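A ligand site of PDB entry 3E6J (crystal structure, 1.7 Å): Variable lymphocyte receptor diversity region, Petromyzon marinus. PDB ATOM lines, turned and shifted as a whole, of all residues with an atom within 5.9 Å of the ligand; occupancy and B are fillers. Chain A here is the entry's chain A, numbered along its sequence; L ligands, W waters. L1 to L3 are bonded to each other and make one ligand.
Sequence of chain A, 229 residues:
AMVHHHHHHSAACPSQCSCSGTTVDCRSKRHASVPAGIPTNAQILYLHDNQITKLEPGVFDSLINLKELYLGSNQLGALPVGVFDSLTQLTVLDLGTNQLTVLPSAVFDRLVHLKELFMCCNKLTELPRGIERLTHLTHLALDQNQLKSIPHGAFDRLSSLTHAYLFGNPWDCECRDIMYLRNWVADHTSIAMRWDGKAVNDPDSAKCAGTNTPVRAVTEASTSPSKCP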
ATOM      1  N   TYR A  46     -12.840   8.925  21.877  1.00  0.00           N
ATOM      2  CA  TYR A  46     -13.954   9.656  21.290  1.00  0.00           C
ATOM      3  C   TYR A  46     -13.949   9.437  19.792  1.00  0.00           C
ATOM      4  O   TYR A  46     -13.057   9.845  19.078  1.00  0.00           O
ATOM      5  CB  TYR A  46     -13.845  11.145  21.556  1.00  0.00           C
ATOM      6  CG  TYR A  46     -13.804  11.576  23.013  1.00  0.00           C
ATOM      7  CD1 TYR A  46     -14.958  11.572  23.766  1.00  0.00           C
ATOM      8  CD2 TYR A  46     -12.638  12.033  23.578  1.00  0.00           C
ATOM      9  CE1 TYR A  46     -14.927  11.948  25.070  1.00  0.00           C
ATOM     10  CE2 TYR A  46     -12.608  12.445  24.902  1.00  0.00           C
ATOM     11  CZ  TYR A  46     -13.769  12.406  25.629  1.00  0.00           C
ATOM     12  OH  TYR A  46     -13.799  12.795  26.947  1.00  0.00           O
ATOM     13  N   HIS A  48     -17.193   9.843  18.350  1.00  0.00           N
ATOM     14  CA  HIS A  48     -18.549  10.336  18.079  1.00  0.00           C
ATOM     15  C   HIS A  48     -18.612  11.463  17.059  1.00  0.00           C
ATOM     16  O   HIS A  48     -17.625  12.138  16.774  1.00  0.00           O
ATOM     17  CB  HIS A  48     -19.279  10.738  19.359  1.00  0.00           C
ATOM     18  CG  HIS A  48     -18.682  11.910  20.081  1.00  0.00           C
ATOM     19  ND1 HIS A  48     -17.492  11.821  20.782  1.00  0.00           N
ATOM     20  CD2 HIS A  48     -19.120  13.172  20.230  1.00  0.00           C
ATOM     21  CE1 HIS A  48     -17.232  12.992  21.350  1.00  0.00           C
ATOM     22  NE2 HIS A  48     -18.199  13.837  21.021  1.00  0.00           N
ATOM     23  N   TYR A  70     -16.878   6.276  23.113  1.00  0.00           N
ATOM     24  CA  TYR A  70     -17.962   7.085  22.511  1.00  0.00           C
ATOM     25  C   TYR A  70     -18.073   6.919  21.002  1.00  0.00           C
ATOM     26  O   TYR A  70     -17.220   7.325  20.240  1.00  0.00           O
ATOM     27  CB  TYR A  70     -17.749   8.563  22.871  1.00  0.00           C
ATOM     28  CG  TYR A  70     -17.689   8.787  24.369  1.00  0.00           C
ATOM     29  CD1 TYR A  70     -18.864   8.977  25.115  1.00  0.00           C
ATOM     30  CD2 TYR A  70     -16.471   8.860  25.031  1.00  0.00           C
ATOM     31  CE1 TYR A  70     -18.821   9.174  26.470  1.00  0.00           C
ATOM     32  CE2 TYR A  70     -16.424   9.079  26.415  1.00  0.00           C
ATOM     33  CZ  TYR A  70     -17.594   9.242  27.121  1.00  0.00           C
ATOM     34  OH  TYR A  70     -17.568   9.453  28.484  1.00  0.00           O
ATOM     35  N   SER A  73     -23.665   9.134  17.345  1.00  0.00           N
ATOM     36  CA  SER A  73     -23.802   9.964  16.138  1.00  0.00           C
ATOM     37  C   SER A  73     -22.866   9.508  15.014  1.00  0.00           C
ATOM     38  O   SER A  73     -22.043  10.277  14.461  1.00  0.00           O
ATOM     39  CB  SER A  73     -23.583  11.446  16.492  1.00  0.00           C
ATOM     40  OG  SER A  73     -24.633  11.960  17.299  1.00  0.00           O
ATOM     41  N   ASP A  94     -21.135   4.611  24.795  1.00  0.00           N
ATOM     42  CA  ASP A  94     -22.202   5.432  24.142  1.00  0.00           C
ATOM     43  C   ASP A  94     -22.353   4.978  22.708  1.00  0.00           C
ATOM     44  O   ASP A  94     -21.433   5.087  21.904  1.00  0.00           O
ATOM     45  CB  ASP A  94     -21.828   6.900  24.220  1.00  0.00           C
ATOM     46  CG  ASP A  94     -22.953   7.880  23.778  1.00  0.00           C
ATOM     47  OD1 ASP A  94     -24.040   7.428  23.339  1.00  0.00           O
ATOM     48  OD2 ASP A  94     -22.726   9.130  23.880  1.00  0.00           O
ATOM     49  N   THR A  97     -27.662   7.440  18.829  1.00  0.00           N
ATOM     50  CA  THR A  97     -27.750   8.076  17.497  1.00  0.00           C
ATOM     51  C   THR A  97     -26.906   7.314  16.464  1.00  0.00           C
ATOM     52  O   THR A  97     -25.926   7.803  15.854  1.00  0.00           O
ATOM     53  CB  THR A  97     -27.443   9.598  17.535  1.00  0.00           C
ATOM     54  OG1 THR A  97     -28.208  10.202  18.602  1.00  0.00           O
ATOM     55  CG2 THR A  97     -27.807  10.307  16.155  1.00  0.00           C
ATOM     56  N   PHE A 118     -25.409   4.142  27.040  1.00  0.00           N
ATOM     57  CA  PHE A 118     -26.293   5.057  26.309  1.00  0.00           C
ATOM     58  C   PHE A 118     -26.597   4.502  24.931  1.00  0.00           C
ATOM     59  O   PHE A 118     -25.701   4.272  24.114  1.00  0.00           O
ATOM     60  CB  PHE A 118     -25.650   6.422  26.155  1.00  0.00           C
ATOM     61  CG  PHE A 118     -25.174   7.026  27.449  1.00  0.00           C
ATOM     62  CD1 PHE A 118     -26.091   7.430  28.403  1.00  0.00           C
ATOM     63  CD2 PHE A 118     -23.835   7.172  27.727  1.00  0.00           C
ATOM     64  CE1 PHE A 118     -25.709   7.977  29.586  1.00  0.00           C
ATOM     65  CE2 PHE A 118     -23.435   7.714  28.935  1.00  0.00           C
ATOM     66  CZ  PHE A 118     -24.382   8.110  29.860  1.00  0.00           C
ATOM     67  N   CYS A 120     -29.716   5.711  23.025  1.00  0.00           N
ATOM     68  CA  CYS A 120     -30.880   6.414  22.451  1.00  0.00           C
ATOM     69  C   CYS A 120     -30.834   6.434  20.953  1.00  0.00           C
ATOM     70  O   CYS A 120     -29.807   6.219  20.325  1.00  0.00           O
ATOM     71  CB  CYS A 120     -30.954   7.869  22.929  1.00  0.00           C
ATOM     72  SG  CYS A 120     -29.845   8.954  22.026  1.00  0.00           S
ATOM     73  N   CYS A 121     -31.972   6.746  20.364  1.00  0.00           N
ATOM     74  CA  CYS A 121     -31.999   7.230  19.009  1.00  0.00           C
ATOM     75  C   CYS A 121     -31.408   6.190  18.062  1.00  0.00           C
ATOM     76  O   CYS A 121     -30.644   6.507  17.132  1.00  0.00           O
ATOM     77  CB  CYS A 121     -31.220   8.532  18.905  1.00  0.00           C
ATOM     78  SG  CYS A 121     -31.863   9.841  20.034  1.00  0.00           S
ATOM     79  N   HIS A 139     -26.216   4.828  34.880  1.00  0.00           N
ATOM     80  CA  HIS A 139     -26.940   5.530  33.821  1.00  0.00           C
ATOM     81  C   HIS A 139     -27.289   4.573  32.676  1.00  0.00           C
ATOM     82  O   HIS A 139     -26.442   3.818  32.216  1.00  0.00           O
ATOM     83  CB  HIS A 139     -26.122   6.644  33.188  1.00  0.00           C
ATOM     84  CG  HIS A 139     -25.808   7.794  34.087  1.00  0.00           C
ATOM     85  ND1 HIS A 139     -25.073   7.638  35.238  1.00  0.00           N
ATOM     86  CD2 HIS A 139     -26.018   9.120  33.939  1.00  0.00           C
ATOM     87  CE1 HIS A 139     -24.904   8.821  35.808  1.00  0.00           C
ATOM     88  NE2 HIS A 139     -25.462   9.739  35.038  1.00  0.00           N
ATOM     89  N   ALA A 141     -29.633   4.787  29.020  1.00  0.00           N
ATOM     90  CA  ALA A 141     -30.459   5.580  28.126  1.00  0.00           C
ATOM     91  C   ALA A 141     -31.005   4.740  26.982  1.00  0.00           C
ATOM     92  O   ALA A 141     -30.239   4.166  26.188  1.00  0.00           O
ATOM     93  CB  ALA A 141     -29.673   6.787  27.605  1.00  0.00           C
ATOM     94  N   LEU A 142     -32.308   4.626  26.966  1.00  0.00           N
ATOM     95  CA  LEU A 142     -33.050   3.864  25.928  1.00  0.00           C
ATOM     96  C   LEU A 142     -34.035   4.710  25.173  1.00  0.00           C
ATOM     97  O   LEU A 142     -34.845   4.212  24.385  1.00  0.00           O
ATOM     98  CB  LEU A 142     -33.774   2.695  26.566  1.00  0.00           C
ATOM     99  CG  LEU A 142     -32.903   1.664  27.306  1.00  0.00           C
ATOM    100  CD1 LEU A 142     -33.832   0.812  28.192  1.00  0.00           C
ATOM    101  CD2 LEU A 142     -32.071   0.849  26.346  1.00  0.00           C
ATOM    102  N   ASP A 143     -33.967   6.026  25.350  1.00  0.00           N
ATOM    103  CA  ASP A 143     -34.927   6.947  24.729  1.00  0.00           C
ATOM    104  C   ASP A 143     -34.930   6.930  23.211  1.00  0.00           C
ATOM    105  O   ASP A 143     -33.922   6.672  22.571  1.00  0.00           O
ATOM    106  CB  ASP A 143     -34.765   8.377  25.247  1.00  0.00           C
ATOM    107  CG  ASP A 143     -33.320   8.905  25.148  1.00  0.00           C
ATOM    108  OD1 ASP A 143     -32.453   8.413  25.934  1.00  0.00           O
ATOM    109  OD2 ASP A 143     -33.081   9.807  24.310  1.00  0.00           O
ATOM    110  N   GLN A 144     -36.101   7.209  22.660  1.00  0.00           N
ATOM    111  CA  GLN A 144     -36.238   7.471  21.217  1.00  0.00           C
ATOM    112  C   GLN A 144     -35.812   6.274  20.384  1.00  0.00           C
ATOM    113  O   GLN A 144     -35.081   6.359  19.380  1.00  0.00           O
ATOM    114  CB  GLN A 144     -35.436   8.696  20.805  1.00  0.00           C
ATOM    115  CG  GLN A 144     -35.829   9.979  21.572  1.00  0.00           C
ATOM    116  CD  GLN A 144     -34.966  11.165  21.274  1.00  0.00           C
ATOM    117  OE1 GLN A 144     -35.097  11.808  20.222  1.00  0.00           O
ATOM    118  NE2 GLN A 144     -34.110  11.519  22.218  1.00  0.00           N
ATOM    119  N   TYR A 165     -33.400   6.836  31.098  1.00  0.00           N
ATOM    120  CA  TYR A 165     -34.100   7.565  30.073  1.00  0.00           C
ATOM    121  C   TYR A 165     -34.935   6.605  29.216  1.00  0.00           C
ATOM    122  O   TYR A 165     -34.394   5.734  28.521  1.00  0.00           O
ATOM    123  CB  TYR A 165     -33.119   8.296  29.161  1.00  0.00           C
ATOM    124  CG  TYR A 165     -32.133   9.203  29.873  1.00  0.00           C
ATOM    125  CD1 TYR A 165     -31.013   8.704  30.455  1.00  0.00           C
ATOM    126  CD2 TYR A 165     -32.351  10.577  29.915  1.00  0.00           C
ATOM    127  CE1 TYR A 165     -30.115   9.513  31.109  1.00  0.00           C
ATOM    128  CE2 TYR A 165     -31.445  11.413  30.562  1.00  0.00           C
ATOM    129  CZ  TYR A 165     -30.352  10.875  31.142  1.00  0.00           C
ATOM    130  OH  TYR A 165     -29.464  11.743  31.750  1.00  0.00           O
ATOM    131  N   PHE A 167     -38.184   7.890  27.671  1.00  0.00           N
ATOM    132  CA  PHE A 167     -39.060   8.686  26.793  1.00  0.00           C
ATOM    133  C   PHE A 167     -38.846   8.398  25.317  1.00  0.00           C
ATOM    134  O   PHE A 167     -37.847   7.798  24.888  1.00  0.00           O
ATOM    135  CB  PHE A 167     -38.916  10.186  27.081  1.00  0.00           C
ATOM    136  CG  PHE A 167     -37.594  10.750  26.658  1.00  0.00           C
ATOM    137  CD1 PHE A 167     -36.500  10.822  27.540  1.00  0.00           C
ATOM    138  CD2 PHE A 167     -37.452  11.246  25.381  1.00  0.00           C
ATOM    139  CE1 PHE A 167     -35.295  11.323  27.098  1.00  0.00           C
ATOM    140  CE2 PHE A 167     -36.242  11.733  24.948  1.00  0.00           C
ATOM    141  CZ  PHE A 167     -35.170  11.797  25.808  1.00  0.00           C
ATOM    142  N   TRP A 195     -34.928  14.651  28.691  1.00  0.00           N
ATOM    143  CA  TRP A 195     -33.798  15.431  28.188  1.00  0.00           C
ATOM    144  C   TRP A 195     -34.183  16.783  27.652  1.00  0.00           C
ATOM    145  O   TRP A 195     -34.772  16.898  26.586  1.00  0.00           O
ATOM    146  CB  TRP A 195     -33.069  14.671  27.074  1.00  0.00           C
ATOM    147  CG  TRP A 195     -31.742  15.268  26.744  1.00  0.00           C
ATOM    148  CD1 TRP A 195     -31.416  16.035  25.675  1.00  0.00           C
ATOM    149  CD2 TRP A 195     -30.539  15.084  27.502  1.00  0.00           C
ATOM    150  NE1 TRP A 195     -30.084  16.354  25.717  1.00  0.00           N
ATOM    151  CE2 TRP A 195     -29.523  15.789  26.831  1.00  0.00           C
ATOM    152  CE3 TRP A 195     -30.220  14.389  28.668  1.00  0.00           C
ATOM    153  CZ2 TRP A 195     -28.226  15.859  27.315  1.00  0.00           C
ATOM    154  CZ3 TRP A 195     -28.934  14.442  29.132  1.00  0.00           C
ATOM    155  CH2 TRP A 195     -27.956  15.181  28.464  1.00  0.00           C
ATOM    156  N   GLY A 197     -32.035  19.155  26.881  1.00  0.00           N
ATOM    157  CA  GLY A 197     -30.653  19.547  26.610  1.00  0.00           C
ATOM    158  C   GLY A 197     -29.741  19.223  27.770  1.00  0.00           C
ATOM    159  O   GLY A 197     -28.556  19.533  27.770  1.00  0.00           O
HETATM  160  C1  LIG L   1     -23.455  14.177  23.529  1.00  0.00           C
HETATM  161  C2  LIG L   1     -23.148  12.926  24.299  1.00  0.00           C
HETATM  162  C3  LIG L   1     -24.426  12.161  23.963  1.00  0.00           C
HETATM  163  C4  LIG L   1     -25.653  13.032  24.313  1.00  0.00           C
HETATM  164  C5  LIG L   1     -25.582  14.401  23.641  1.00  0.00           C
HETATM  165  C6  LIG L   1     -26.767  15.282  23.988  1.00  0.00           C
HETATM  166  C7  LIG L   1     -20.836  12.441  24.449  1.00  0.00           C
HETATM  167  C8  LIG L   1     -19.580  11.937  23.834  1.00  0.00           C
HETATM  168  N1  LIG L   1     -21.952  12.355  23.738  1.00  0.00           N
HETATM  169  O1  LIG L   1     -23.118  14.379  22.163  1.00  0.00           O
HETATM  170  O2  LIG L   1     -24.476  10.913  24.650  1.00  0.00           O
HETATM  171  O3  LIG L   1     -26.817  12.285  23.884  1.00  0.00           O
HETATM  172  O4  LIG L   1     -24.393  15.079  24.066  1.00  0.00           O
HETATM  173  O5  LIG L   1     -26.649  16.462  23.178  1.00  0.00           O
HETATM  174  O6  LIG L   1     -20.865  12.895  25.563  1.00  0.00           O
HETATM  175  C1  LG2 L   2     -27.855  12.361  24.850  1.00  0.00           C
HETATM  176  C2  LG2 L   2     -29.218  12.141  24.197  1.00  0.00           C
HETATM  177  C3  LG2 L   2     -30.344  12.147  25.236  1.00  0.00           C
HETATM  178  C4  LG2 L   2     -30.084  11.087  26.287  1.00  0.00           C
HETATM  179  C5  LG2 L   2     -28.674  11.303  26.834  1.00  0.00           C
HETATM  180  C6  LG2 L   2     -28.269  10.273  27.867  1.00  0.00           C
HETATM  181  O1  LG2 L   2     -29.459  13.173  23.232  1.00  0.00           O
HETATM  182  O2  LG2 L   2     -31.577  11.922  24.533  1.00  0.00           O
HETATM  183  O3  LG2 L   2     -30.142   9.758  25.713  1.00  0.00           O
HETATM  184  O4  LG2 L   2     -27.670  11.309  25.772  1.00  0.00           O
HETATM  185  O5  LG2 L   2     -27.203  10.852  28.630  1.00  0.00           O
HETATM  186  C1  LG3 L   3     -29.921  12.775  21.952  1.00  0.00           C
HETATM  187  C2  LG3 L   3     -31.018  13.731  21.506  1.00  0.00           C
HETATM  188  C3  LG3 L   3     -30.379  15.109  21.343  1.00  0.00           C
HETATM  189  C4  LG3 L   3     -29.222  15.069  20.326  1.00  0.00           C
HETATM  190  C5  LG3 L   3     -28.194  14.032  20.740  1.00  0.00           C
HETATM  191  C6  LG3 L   3     -27.066  13.878  19.719  1.00  0.00           C
HETATM  192  O1  LG3 L   3     -32.098  13.715  22.485  1.00  0.00           O
HETATM  193  O2  LG3 L   3     -31.346  16.084  20.959  1.00  0.00           O
HETATM  194  O3  LG3 L   3     -29.766  14.730  19.040  1.00  0.00           O
HETATM  195  O4  LG3 L   3     -28.836  12.772  20.996  1.00  0.00           O
HETATM  196  O   HOH W   1     -22.283  16.443  20.862  1.00  0.00           O
HETATM  197  O   HOH W   2     -27.024  10.478  21.054  1.00  0.00           O
HETATM  198  O   HOH W   3     -22.233  11.710  20.851  1.00  0.00           O
HETATM  199  O   HOH W   4     -18.704  12.569  27.723  1.00  0.00           O
HETATM  200  O   HOH W   5     -22.408  13.993  19.114  1.00  0.00           O
HETATM  201  O   HOH W   6     -24.615  10.878  27.369  1.00  0.00           O
HETATM  202  O   HOH W   7     -34.032  15.760  22.609  1.00  0.00           O
HETATM  203  O   HOH W   8     -28.585  16.424  17.278  1.00  0.00           O
HETATM  204  O   HOH W   9     -26.962  10.946  31.300  1.00  0.00           O
HETATM  205  O   HOH W  10     -28.325   7.836  24.623  1.00  0.00           O
HETATM  206  O   HOH W  11     -32.775  15.754  18.585  1.00  0.00           O
HETATM  207  O   HOH W  12     -30.131  12.174  17.985  1.00  0.00           O
HETATM  208  O   HOH W  13     -26.120   9.128  23.474  1.00  0.00           O
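An oxygen (O2) of LG2 L2 sits at hydrogen-bond distance from the side-chain carboxylate (OD2) of Asp 143, at 2.6 Å. The side-chain carboxylate (OD2) of Asp 94 lies within hydrogen-bond range of an oxygen (O2) of LIG L1, 2.6 Å away. The side-chain amide nitrogen (NE2) of Gln 144 sits at hydrogen-bond distance from an oxygen (O1) of LG3 L3, at 3.0 Å. An oxygen (O3) of LG2 L2 sits close to the side-chain sulfur (SG) of Cys 120, at 3.8 Å.
The side-chain carboxylate (OD2) of Asp 143 lies within hydrogen-bond range of the side-chain amide nitrogen (NE2) of Gln 144. N of Asp 143 is in hydrogen-bond range of O of Tyr 165 (3.2 Å). N of Cys 121 lies within hydrogen-bond range of O of Asp 143. The backbone carbonyl oxygen (O) of Gln 144 lies close to the backbone NH (N) of Cys 121, 3.3 Å away. N of His 48 sits at hydrogen-bond distance from O of Tyr 70 (3.1 Å). N of Thr 97 sits at hydrogen-bond distance from O of Cys 120, 2.9 Å away. The backbone NH (N) of Ser 73 lies within hydrogen-bond range of the backbone carbonyl oxygen (O) of Thr 97, 3.0 Å away. O of Tyr 165 lies within hydrogen-bond range of N of Leu 142, 2.8 Å away.
Residues that only touch the ligand: His 48, Tyr 70, Ser 73, Thr 97, Phe 118, Ala 141, Tyr 165, Phe 167 and Trp 195. Hydrophobic or aromatic side chains within 4 Å of the ligand: His 48, Tyr 70, Phe 118, Ala 141, Tyr 165, Phe 167 and Trp 195. Of the 18 residues printed, 13 come within 4 Å of the ligand. The nearest printed residue that does not touch the ligand is Cys 121 (4.01 Å).
Water W9 bridges OH of Tyr 165 and O5 of LG2 L2. Water W13 bridges OD1 of Asp 94 (2.7 Å) and O2 of LIG L1 (2.7 Å). Water W12 lies within hydrogen-bond range of O3 of LG3 L3 (2.8 Å), OG1 of Thr 97 (2.8 Å) and SG of Cys 121 (3.6 Å). Water W10 bridges an oxygen (O3) of LG2 L2 (2.9 Å) and the backbone NH (N) of Cys 120 (3.0 Å). Water W2 lies within hydrogen-bond range of OG1 of Thr 97 (2.7 Å), O4 of LG3 L3 (2.9 Å) and SG of Cys 120 (3.4 Å). Water W4 lies within hydrogen-bond range of an oxygen (O6) of LIG L1 and the side-chain hydroxyl (OH) of Tyr 70.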
